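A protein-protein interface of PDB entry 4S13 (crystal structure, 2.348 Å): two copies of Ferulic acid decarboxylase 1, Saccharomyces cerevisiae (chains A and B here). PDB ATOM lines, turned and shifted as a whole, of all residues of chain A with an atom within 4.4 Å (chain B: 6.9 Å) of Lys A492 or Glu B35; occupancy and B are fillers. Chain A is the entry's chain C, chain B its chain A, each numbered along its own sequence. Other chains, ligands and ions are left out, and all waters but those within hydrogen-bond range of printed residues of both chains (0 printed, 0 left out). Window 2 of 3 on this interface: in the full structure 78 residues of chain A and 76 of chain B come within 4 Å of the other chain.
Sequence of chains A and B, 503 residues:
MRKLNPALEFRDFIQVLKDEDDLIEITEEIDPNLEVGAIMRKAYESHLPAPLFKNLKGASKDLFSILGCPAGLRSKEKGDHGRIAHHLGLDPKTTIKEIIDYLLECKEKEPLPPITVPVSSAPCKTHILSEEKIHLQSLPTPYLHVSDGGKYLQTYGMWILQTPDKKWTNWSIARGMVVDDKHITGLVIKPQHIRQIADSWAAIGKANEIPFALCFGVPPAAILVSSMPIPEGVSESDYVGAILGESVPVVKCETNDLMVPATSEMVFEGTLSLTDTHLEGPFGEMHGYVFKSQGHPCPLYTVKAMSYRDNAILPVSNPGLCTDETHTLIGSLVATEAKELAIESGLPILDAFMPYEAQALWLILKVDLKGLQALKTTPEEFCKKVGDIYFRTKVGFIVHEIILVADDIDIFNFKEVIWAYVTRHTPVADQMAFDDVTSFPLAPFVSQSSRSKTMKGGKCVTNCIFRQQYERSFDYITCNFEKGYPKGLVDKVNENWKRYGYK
OE2 of Glu B35 is in salt-bridge range of NZ of Lys A492, 3.1 Å away.
The backbone NH (N) of Asp B31 sits at hydrogen-bond distance from the side-chain carboxylate (OE1) of Glu B35, 2.9 Å away. O of Tyr B143 lies within hydrogen-bond range of N of Leu B34, 3.0 Å away.
Leu B34 touches Leu A489 (CB to CD2, 3.5 Å). CD1 of Leu A489 touches CG of Glu B35, 3.6 Å away. CG1 of Ile B39 touches CG1 of Val A493 (3.9 Å).
Of the printed residues of chain B, Leu A489 touches Leu B34 and Glu B35. Of chain B, only Glu B35 comes within 4 Å of Lys A492. Of the printed residues of chain B, Val A493 touches Ile B39. Glu A495 touches none of the printed residues of chain B. Of the printed residues of chain A, Leu B34 touches Leu A489. Of chain A, only Leu A489 (3.6 Å) and Lys A492 (3.1 Å) come within 4 Å of Glu B35. Printed residues of chain A within 4 Å of Ile B39: Val A493 (3.9 Å). The nearest printed residue of chain A that does not touch Glu B35 is Val A493 (4.9 Å).
Of the 16 printed residues of chain B, 3 touch a printed residue of chain A. Hydrophobic or aromatic side chains of chain B within 4 Å of the printed part of chain A: Leu B34 and Ile B39. Among the printed residues, Asp or Glu carboxylates within 4 Å of a Lys or Arg side-chain nitrogen of the other chain: Lys A492 with Glu B35 (3.1 Å).
No position is printed for both chains. Of the 4 pairs that touch across the chains among the printed residues, none has its exchanged pair printed and touching as well.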
ATOM      1  N   GLY A 488     -19.117  27.291   9.651  1.00  0.00           N
ATOM      2  CA  GLY A 488     -20.069  26.229   9.440  1.00  0.00           C
ATOM      3  C   GLY A 488     -21.051  26.237  10.574  1.00  0.00           C
ATOM      4  O   GLY A 488     -22.254  26.266  10.342  1.00  0.00           O
ATOM      5  N   LEU A 489     -20.555  26.212  11.807  1.00  0.00           N
ATOM      6  CA  LEU A 489     -21.449  26.472  12.915  1.00  0.00           C
ATOM      7  C   LEU A 489     -21.865  27.921  12.789  1.00  0.00           C
ATOM      8  O   LEU A 489     -23.045  28.225  12.834  1.00  0.00           O
ATOM      9  CB  LEU A 489     -20.809  26.198  14.264  1.00  0.00           C
ATOM     10  CG  LEU A 489     -21.746  26.526  15.432  1.00  0.00           C
ATOM     11  CD1 LEU A 489     -23.152  25.969  15.193  1.00  0.00           C
ATOM     12  CD2 LEU A 489     -21.178  25.979  16.709  1.00  0.00           C
ATOM     13  N   VAL A 490     -20.887  28.804  12.599  1.00  0.00           N
ATOM     14  CA  VAL A 490     -21.166  30.205  12.298  1.00  0.00           C
ATOM     15  C   VAL A 490     -22.146  30.336  11.133  1.00  0.00           C
ATOM     16  O   VAL A 490     -23.177  30.998  11.268  1.00  0.00           O
ATOM     17  CB  VAL A 490     -19.878  30.989  11.956  1.00  0.00           C
ATOM     18  CG1 VAL A 490     -20.212  32.398  11.559  1.00  0.00           C
ATOM     19  CG2 VAL A 490     -18.930  31.011  13.147  1.00  0.00           C
ATOM     20  N   ASP A 491     -21.823  29.705  10.003  1.00  0.00           N
ATOM     21  CA  ASP A 491     -22.680  29.750   8.827  1.00  0.00           C
ATOM     22  C   ASP A 491     -24.101  29.268   9.118  1.00  0.00           C
ATOM     23  O   ASP A 491     -25.057  29.937   8.762  1.00  0.00           O
ATOM     24  CB  ASP A 491     -22.070  28.931   7.688  1.00  0.00           C
ATOM     25  CG  ASP A 491     -20.819  29.573   7.116  1.00  0.00           C
ATOM     26  OD1 ASP A 491     -20.585  30.759   7.424  1.00  0.00           O
ATOM     27  OD2 ASP A 491     -20.080  28.902   6.364  1.00  0.00           O
ATOM     28  N   LYS A 492     -24.233  28.132   9.796  1.00  0.00           N
ATOM     29  CA  LYS A 492     -25.542  27.600  10.163  1.00  0.00           C
ATOM     30  C   LYS A 492     -26.344  28.549  11.054  1.00  0.00           C
ATOM     31  O   LYS A 492     -27.523  28.796  10.807  1.00  0.00           O
ATOM     32  CB  LYS A 492     -25.393  26.260  10.875  1.00  0.00           C
ATOM     33  CG  LYS A 492     -26.719  25.658  11.310  1.00  0.00           C
ATOM     34  CD  LYS A 492     -26.514  24.345  12.032  1.00  0.00           C
ATOM     35  CE  LYS A 492     -27.831  23.742  12.449  1.00  0.00           C
ATOM     36  NZ  LYS A 492     -27.643  22.384  13.006  1.00  0.00           N
ATOM     37  N   VAL A 493     -25.708  29.064  12.098  1.00  0.00           N
ATOM     38  CA  VAL A 493     -26.383  29.962  13.021  1.00  0.00           C
ATOM     39  C   VAL A 493     -26.863  31.214  12.288  1.00  0.00           C
ATOM     40  O   VAL A 493     -27.992  31.657  12.480  1.00  0.00           O
ATOM     41  CB  VAL A 493     -25.469  30.337  14.189  1.00  0.00           C
ATOM     42  CG1 VAL A 493     -26.061  31.474  14.997  1.00  0.00           C
ATOM     43  CG2 VAL A 493     -25.216  29.117  15.059  1.00  0.00           C
ATOM     44  N   ASN A 494     -26.008  31.762  11.430  1.00  0.00           N
ATOM     45  CA  ASN A 494     -26.389  32.881  10.582  1.00  0.00           C
ATOM     46  C   ASN A 494     -27.535  32.568   9.638  1.00  0.00           C
ATOM     47  O   ASN A 494     -28.393  33.407   9.412  1.00  0.00           O
ATOM     48  CB  ASN A 494     -25.193  33.362   9.765  1.00  0.00           C
ATOM     49  CG  ASN A 494     -24.208  34.113  10.604  1.00  0.00           C
ATOM     50  OD1 ASN A 494     -24.548  34.577  11.692  1.00  0.00           O
ATOM     51  ND2 ASN A 494     -22.975  34.237  10.116  1.00  0.00           N
ATOM     52  N   GLU A 495     -27.530  31.368   9.076  1.00  0.00           N
ATOM     53  CA  GLU A 495     -28.569  30.943   8.162  1.00  0.00           C
ATOM     54  C   GLU A 495     -29.926  30.878   8.845  1.00  0.00           C
ATOM     55  O   GLU A 495     -30.923  31.409   8.348  1.00  0.00           O
ATOM     56  CB  GLU A 495     -28.228  29.577   7.581  1.00  0.00           C
ATOM     57  CG  GLU A 495     -27.685  29.627   6.177  1.00  0.00           C
ATOM     58  CD  GLU A 495     -27.114  28.299   5.739  1.00  0.00           C
ATOM     59  OE1 GLU A 495     -25.910  28.054   5.977  1.00  0.00           O
ATOM     60  OE2 GLU A 495     -27.876  27.497   5.162  1.00  0.00           O
ATOM     61  N   ASN A 496     -29.941  30.214   9.991  1.00  0.00           N
ATOM     62  CA  ASN A 496     -31.156  29.961  10.742  1.00  0.00           C
ATOM     63  C   ASN A 496     -31.589  31.115  11.638  1.00  0.00           C
ATOM     64  O   ASN A 496     -32.596  31.020  12.324  1.00  0.00           O
ATOM     65  CB  ASN A 496     -30.970  28.705  11.579  1.00  0.00           C
ATOM     66  CG  ASN A 496     -30.774  27.475  10.733  1.00  0.00           C
ATOM     67  OD1 ASN A 496     -31.024  27.495   9.539  1.00  0.00           O
ATOM     68  ND2 ASN A 496     -30.324  26.394  11.350  1.00  0.00           N
ATOM     69  N   GLU B  28     -37.027  24.992  17.850  1.00  0.00           N
ATOM     70  CA  GLU B  28     -36.426  23.927  17.072  1.00  0.00           C
ATOM     71  C   GLU B  28     -35.297  23.300  17.866  1.00  0.00           C
ATOM     72  O   GLU B  28     -34.824  23.874  18.835  1.00  0.00           O
ATOM     73  CB  GLU B  28     -35.922  24.440  15.739  1.00  0.00           C
ATOM     74  CG  GLU B  28     -34.709  25.301  15.821  1.00  0.00           C
ATOM     75  CD  GLU B  28     -34.233  25.682  14.444  1.00  0.00           C
ATOM     76  OE1 GLU B  28     -34.982  26.397  13.745  1.00  0.00           O
ATOM     77  OE2 GLU B  28     -33.131  25.237  14.058  1.00  0.00           O
ATOM     78  N   GLU B  29     -34.872  22.119  17.453  1.00  0.00           N
ATOM     79  CA  GLU B  29     -33.852  21.385  18.177  1.00  0.00           C
ATOM     80  C   GLU B  29     -32.499  22.076  18.060  1.00  0.00           C
ATOM     81  O   GLU B  29     -32.050  22.438  16.975  1.00  0.00           O
ATOM     82  CB  GLU B  29     -33.757  19.943  17.673  1.00  0.00           C
ATOM     83  CG  GLU B  29     -33.169  18.984  18.694  1.00  0.00           C
ATOM     84  CD  GLU B  29     -33.188  17.541  18.225  1.00  0.00           C
ATOM     85  OE1 GLU B  29     -34.288  17.010  17.944  1.00  0.00           O
ATOM     86  OE2 GLU B  29     -32.097  16.940  18.137  1.00  0.00           O
ATOM     87  N   ILE B  30     -31.856  22.243  19.202  1.00  0.00           N
ATOM     88  CA  ILE B  30     -30.603  22.948  19.292  1.00  0.00           C
ATOM     89  C   ILE B  30     -29.651  22.109  20.119  1.00  0.00           C
ATOM     90  O   ILE B  30     -30.015  21.612  21.184  1.00  0.00           O
ATOM     91  CB  ILE B  30     -30.802  24.343  19.911  1.00  0.00           C
ATOM     92  CG1 ILE B  30     -31.627  25.232  18.962  1.00  0.00           C
ATOM     93  CG2 ILE B  30     -29.468  24.984  20.235  1.00  0.00           C
ATOM     94  CD1 ILE B  30     -30.896  25.646  17.701  1.00  0.00           C
ATOM     95  N   ASP B  31     -28.439  21.926  19.610  1.00  0.00           N
ATOM     96  CA  ASP B  31     -27.446  21.106  20.277  1.00  0.00           C
ATOM     97  C   ASP B  31     -26.744  21.902  21.380  1.00  0.00           C
ATOM     98  O   ASP B  31     -26.214  22.968  21.126  1.00  0.00           O
ATOM     99  CB  ASP B  31     -26.437  20.579  19.256  1.00  0.00           C
ATOM    100  CG  ASP B  31     -25.676  19.365  19.752  1.00  0.00           C
ATOM    101  OD1 ASP B  31     -25.449  19.253  20.971  1.00  0.00           O
ATOM    102  OD2 ASP B  31     -25.300  18.518  18.921  1.00  0.00           O
ATOM    103  N   PRO B  32     -26.747  21.379  22.611  1.00  0.00           N
ATOM    104  CA  PRO B  32     -26.017  21.988  23.735  1.00  0.00           C
ATOM    105  C   PRO B  32     -24.501  21.992  23.505  1.00  0.00           C
ATOM    106  O   PRO B  32     -23.772  22.756  24.133  1.00  0.00           O
ATOM    107  CB  PRO B  32     -26.385  21.099  24.925  1.00  0.00           C
ATOM    108  CG  PRO B  32     -27.640  20.406  24.516  1.00  0.00           C
ATOM    109  CD  PRO B  32     -27.565  20.231  23.036  1.00  0.00           C
ATOM    110  N   ASN B  33     -24.037  21.149  22.591  1.00  0.00           N
ATOM    111  CA  ASN B  33     -22.643  21.151  22.193  1.00  0.00           C
ATOM    112  C   ASN B  33     -22.390  22.289  21.177  1.00  0.00           C
ATOM    113  O   ASN B  33     -22.829  22.230  20.033  1.00  0.00           O
ATOM    114  CB  ASN B  33     -22.280  19.771  21.641  1.00  0.00           C
ATOM    115  CG  ASN B  33     -20.809  19.601  21.378  1.00  0.00           C
ATOM    116  OD1 ASN B  33     -19.992  20.379  21.830  1.00  0.00           O
ATOM    117  ND2 ASN B  33     -20.464  18.562  20.636  1.00  0.00           N
ATOM    118  N   LEU B  34     -21.728  23.343  21.650  1.00  0.00           N
ATOM    119  CA  LEU B  34     -21.369  24.560  20.899  1.00  0.00           C
ATOM    120  C   LEU B  34     -22.521  25.444  20.401  1.00  0.00           C
ATOM    121  O   LEU B  34     -22.434  26.659  20.509  1.00  0.00           O
ATOM    122  CB  LEU B  34     -20.482  24.205  19.704  1.00  0.00           C
ATOM    123  CG  LEU B  34     -19.142  23.554  20.034  1.00  0.00           C
ATOM    124  CD1 LEU B  34     -18.343  23.372  18.756  1.00  0.00           C
ATOM    125  CD2 LEU B  34     -18.390  24.386  21.061  1.00  0.00           C
ATOM    126  N   GLU B  35     -23.578  24.865  19.841  1.00  0.00           N
ATOM    127  CA  GLU B  35     -24.618  25.682  19.204  1.00  0.00           C
ATOM    128  C   GLU B  35     -25.310  26.667  20.157  1.00  0.00           C
ATOM    129  O   GLU B  35     -25.611  27.788  19.767  1.00  0.00           O
ATOM    130  CB  GLU B  35     -25.674  24.788  18.540  1.00  0.00           C
ATOM    131  CG  GLU B  35     -25.156  23.963  17.377  1.00  0.00           C
ATOM    132  CD  GLU B  35     -26.244  23.135  16.674  1.00  0.00           C
ATOM    133  OE1 GLU B  35     -27.384  23.060  17.189  1.00  0.00           O
ATOM    134  OE2 GLU B  35     -25.949  22.559  15.598  1.00  0.00           O
ATOM    135  N   VAL B  36     -25.563  26.251  21.397  1.00  0.00           N
ATOM    136  CA  VAL B  36     -26.129  27.150  22.401  1.00  0.00           C
ATOM    137  C   VAL B  36     -25.201  28.326  22.654  1.00  0.00           C
ATOM    138  O   VAL B  36     -25.618  29.485  22.684  1.00  0.00           O
ATOM    139  CB  VAL B  36     -26.374  26.432  23.740  1.00  0.00           C
ATOM    140  CG1 VAL B  36     -26.510  27.438  24.899  1.00  0.00           C
ATOM    141  CG2 VAL B  36     -27.585  25.520  23.620  1.00  0.00           C
ATOM    142  N   GLY B  37     -23.928  28.007  22.824  1.00  0.00           N
ATOM    143  CA  GLY B  37     -22.931  29.016  23.121  1.00  0.00           C
ATOM    144  C   GLY B  37     -22.733  30.056  22.030  1.00  0.00           C
ATOM    145  O   GLY B  37     -22.643  31.249  22.307  1.00  0.00           O
ATOM    146  N   ALA B  38     -22.680  29.599  20.790  1.00  0.00           N
ATOM    147  CA  ALA B  38     -22.503  30.480  19.645  1.00  0.00           C
ATOM    148  C   ALA B  38     -23.715  31.380  19.415  1.00  0.00           C
ATOM    149  O   ALA B  38     -23.575  32.561  19.093  1.00  0.00           O
ATOM    150  CB  ALA B  38     -22.208  29.666  18.397  1.00  0.00           C
ATOM    151  N   ILE B  39     -24.908  30.815  19.561  1.00  0.00           N
ATOM    152  CA  ILE B  39     -26.115  31.611  19.440  1.00  0.00           C
ATOM    153  C   ILE B  39     -26.128  32.701  20.544  1.00  0.00           C
ATOM    154  O   ILE B  39     -26.500  33.845  20.295  1.00  0.00           O
ATOM    155  CB  ILE B  39     -27.364  30.702  19.499  1.00  0.00           C
ATOM    156  CG1 ILE B  39     -27.486  29.894  18.206  1.00  0.00           C
ATOM    157  CG2 ILE B  39     -28.640  31.513  19.733  1.00  0.00           C
ATOM    158  CD1 ILE B  39     -28.448  28.727  18.284  1.00  0.00           C
ATOM    159  N   MET B  40     -25.668  32.355  21.741  1.00  0.00           N
ATOM    160  CA  MET B  40     -25.579  33.329  22.829  1.00  0.00           C
ATOM    161  C   MET B  40     -24.584  34.447  22.530  1.00  0.00           C
ATOM    162  O   MET B  40     -24.912  35.618  22.705  1.00  0.00           O
ATOM    163  CB  MET B  40     -25.208  32.645  24.133  1.00  0.00           C
ATOM    164  CG  MET B  40     -26.352  31.871  24.749  1.00  0.00           C
ATOM    165  SD  MET B  40     -25.854  31.001  26.223  1.00  0.00           S
ATOM    166  CE  MET B  40     -25.582  32.391  27.308  1.00  0.00           C
ATOM    167  N   PHE B  53     -33.898  28.462  24.931  1.00  0.00           N
ATOM    168  CA  PHE B  53     -33.898  27.228  24.183  1.00  0.00           C
ATOM    169  C   PHE B  53     -34.856  26.223  24.826  1.00  0.00           C
ATOM    170  O   PHE B  53     -34.572  25.683  25.889  1.00  0.00           O
ATOM    171  CB  PHE B  53     -32.487  26.648  24.109  1.00  0.00           C
ATOM    172  CG  PHE B  53     -31.427  27.634  23.645  1.00  0.00           C
ATOM    173  CD1 PHE B  53     -31.152  27.794  22.294  1.00  0.00           C
ATOM    174  CD2 PHE B  53     -30.693  28.380  24.562  1.00  0.00           C
ATOM    175  CE1 PHE B  53     -30.177  28.686  21.870  1.00  0.00           C
ATOM    176  CE2 PHE B  53     -29.706  29.275  24.141  1.00  0.00           C
ATOM    177  CZ  PHE B  53     -29.446  29.420  22.791  1.00  0.00           C
ATOM    178  N   TYR B 143     -21.915  22.740  26.333  1.00  0.00           N
ATOM    179  CA  TYR B 143     -20.478  22.855  26.101  1.00  0.00           C
ATOM    180  C   TYR B 143     -20.260  24.191  25.402  1.00  0.00           C
ATOM    181  O   TYR B 143     -20.510  24.324  24.209  1.00  0.00           O
ATOM    182  CB  TYR B 143     -19.964  21.687  25.258  1.00  0.00           C
ATOM    183  CG  TYR B 143     -18.475  21.672  25.053  1.00  0.00           C
ATOM    184  CD1 TYR B 143     -17.614  21.417  26.110  1.00  0.00           C
ATOM    185  CD2 TYR B 143     -17.931  21.899  23.805  1.00  0.00           C
ATOM    186  CE1 TYR B 143     -16.253  21.402  25.928  1.00  0.00           C
ATOM    187  CE2 TYR B 143     -16.578  21.887  23.611  1.00  0.00           C
ATOM    188  CZ  TYR B 143     -15.740  21.640  24.677  1.00  0.00           C
ATOM    189  OH  TYR B 143     -14.386  21.628  24.485  1.00  0.00           O
ATOM    190  N   LEU B 144     -19.822  25.194  26.154  1.00  0.00           N
ATOM    191  CA  LEU B 144     -20.017  26.574  25.728  1.00  0.00           C
ATOM    192  C   LEU B 144     -18.980  27.146  24.755  1.00  0.00           C
ATOM    193  O   LEU B 144     -19.352  27.882  23.847  1.00  0.00           O
ATOM    194  CB  LEU B 144     -20.108  27.461  26.954  1.00  0.00           C
ATOM    195  CG  LEU B 144     -21.391  27.199  27.730  1.00  0.00           C
ATOM    196  CD1 LEU B 144     -21.309  27.851  29.071  1.00  0.00           C
ATOM    197  CD2 LEU B 144     -22.594  27.724  26.938  1.00  0.00           C
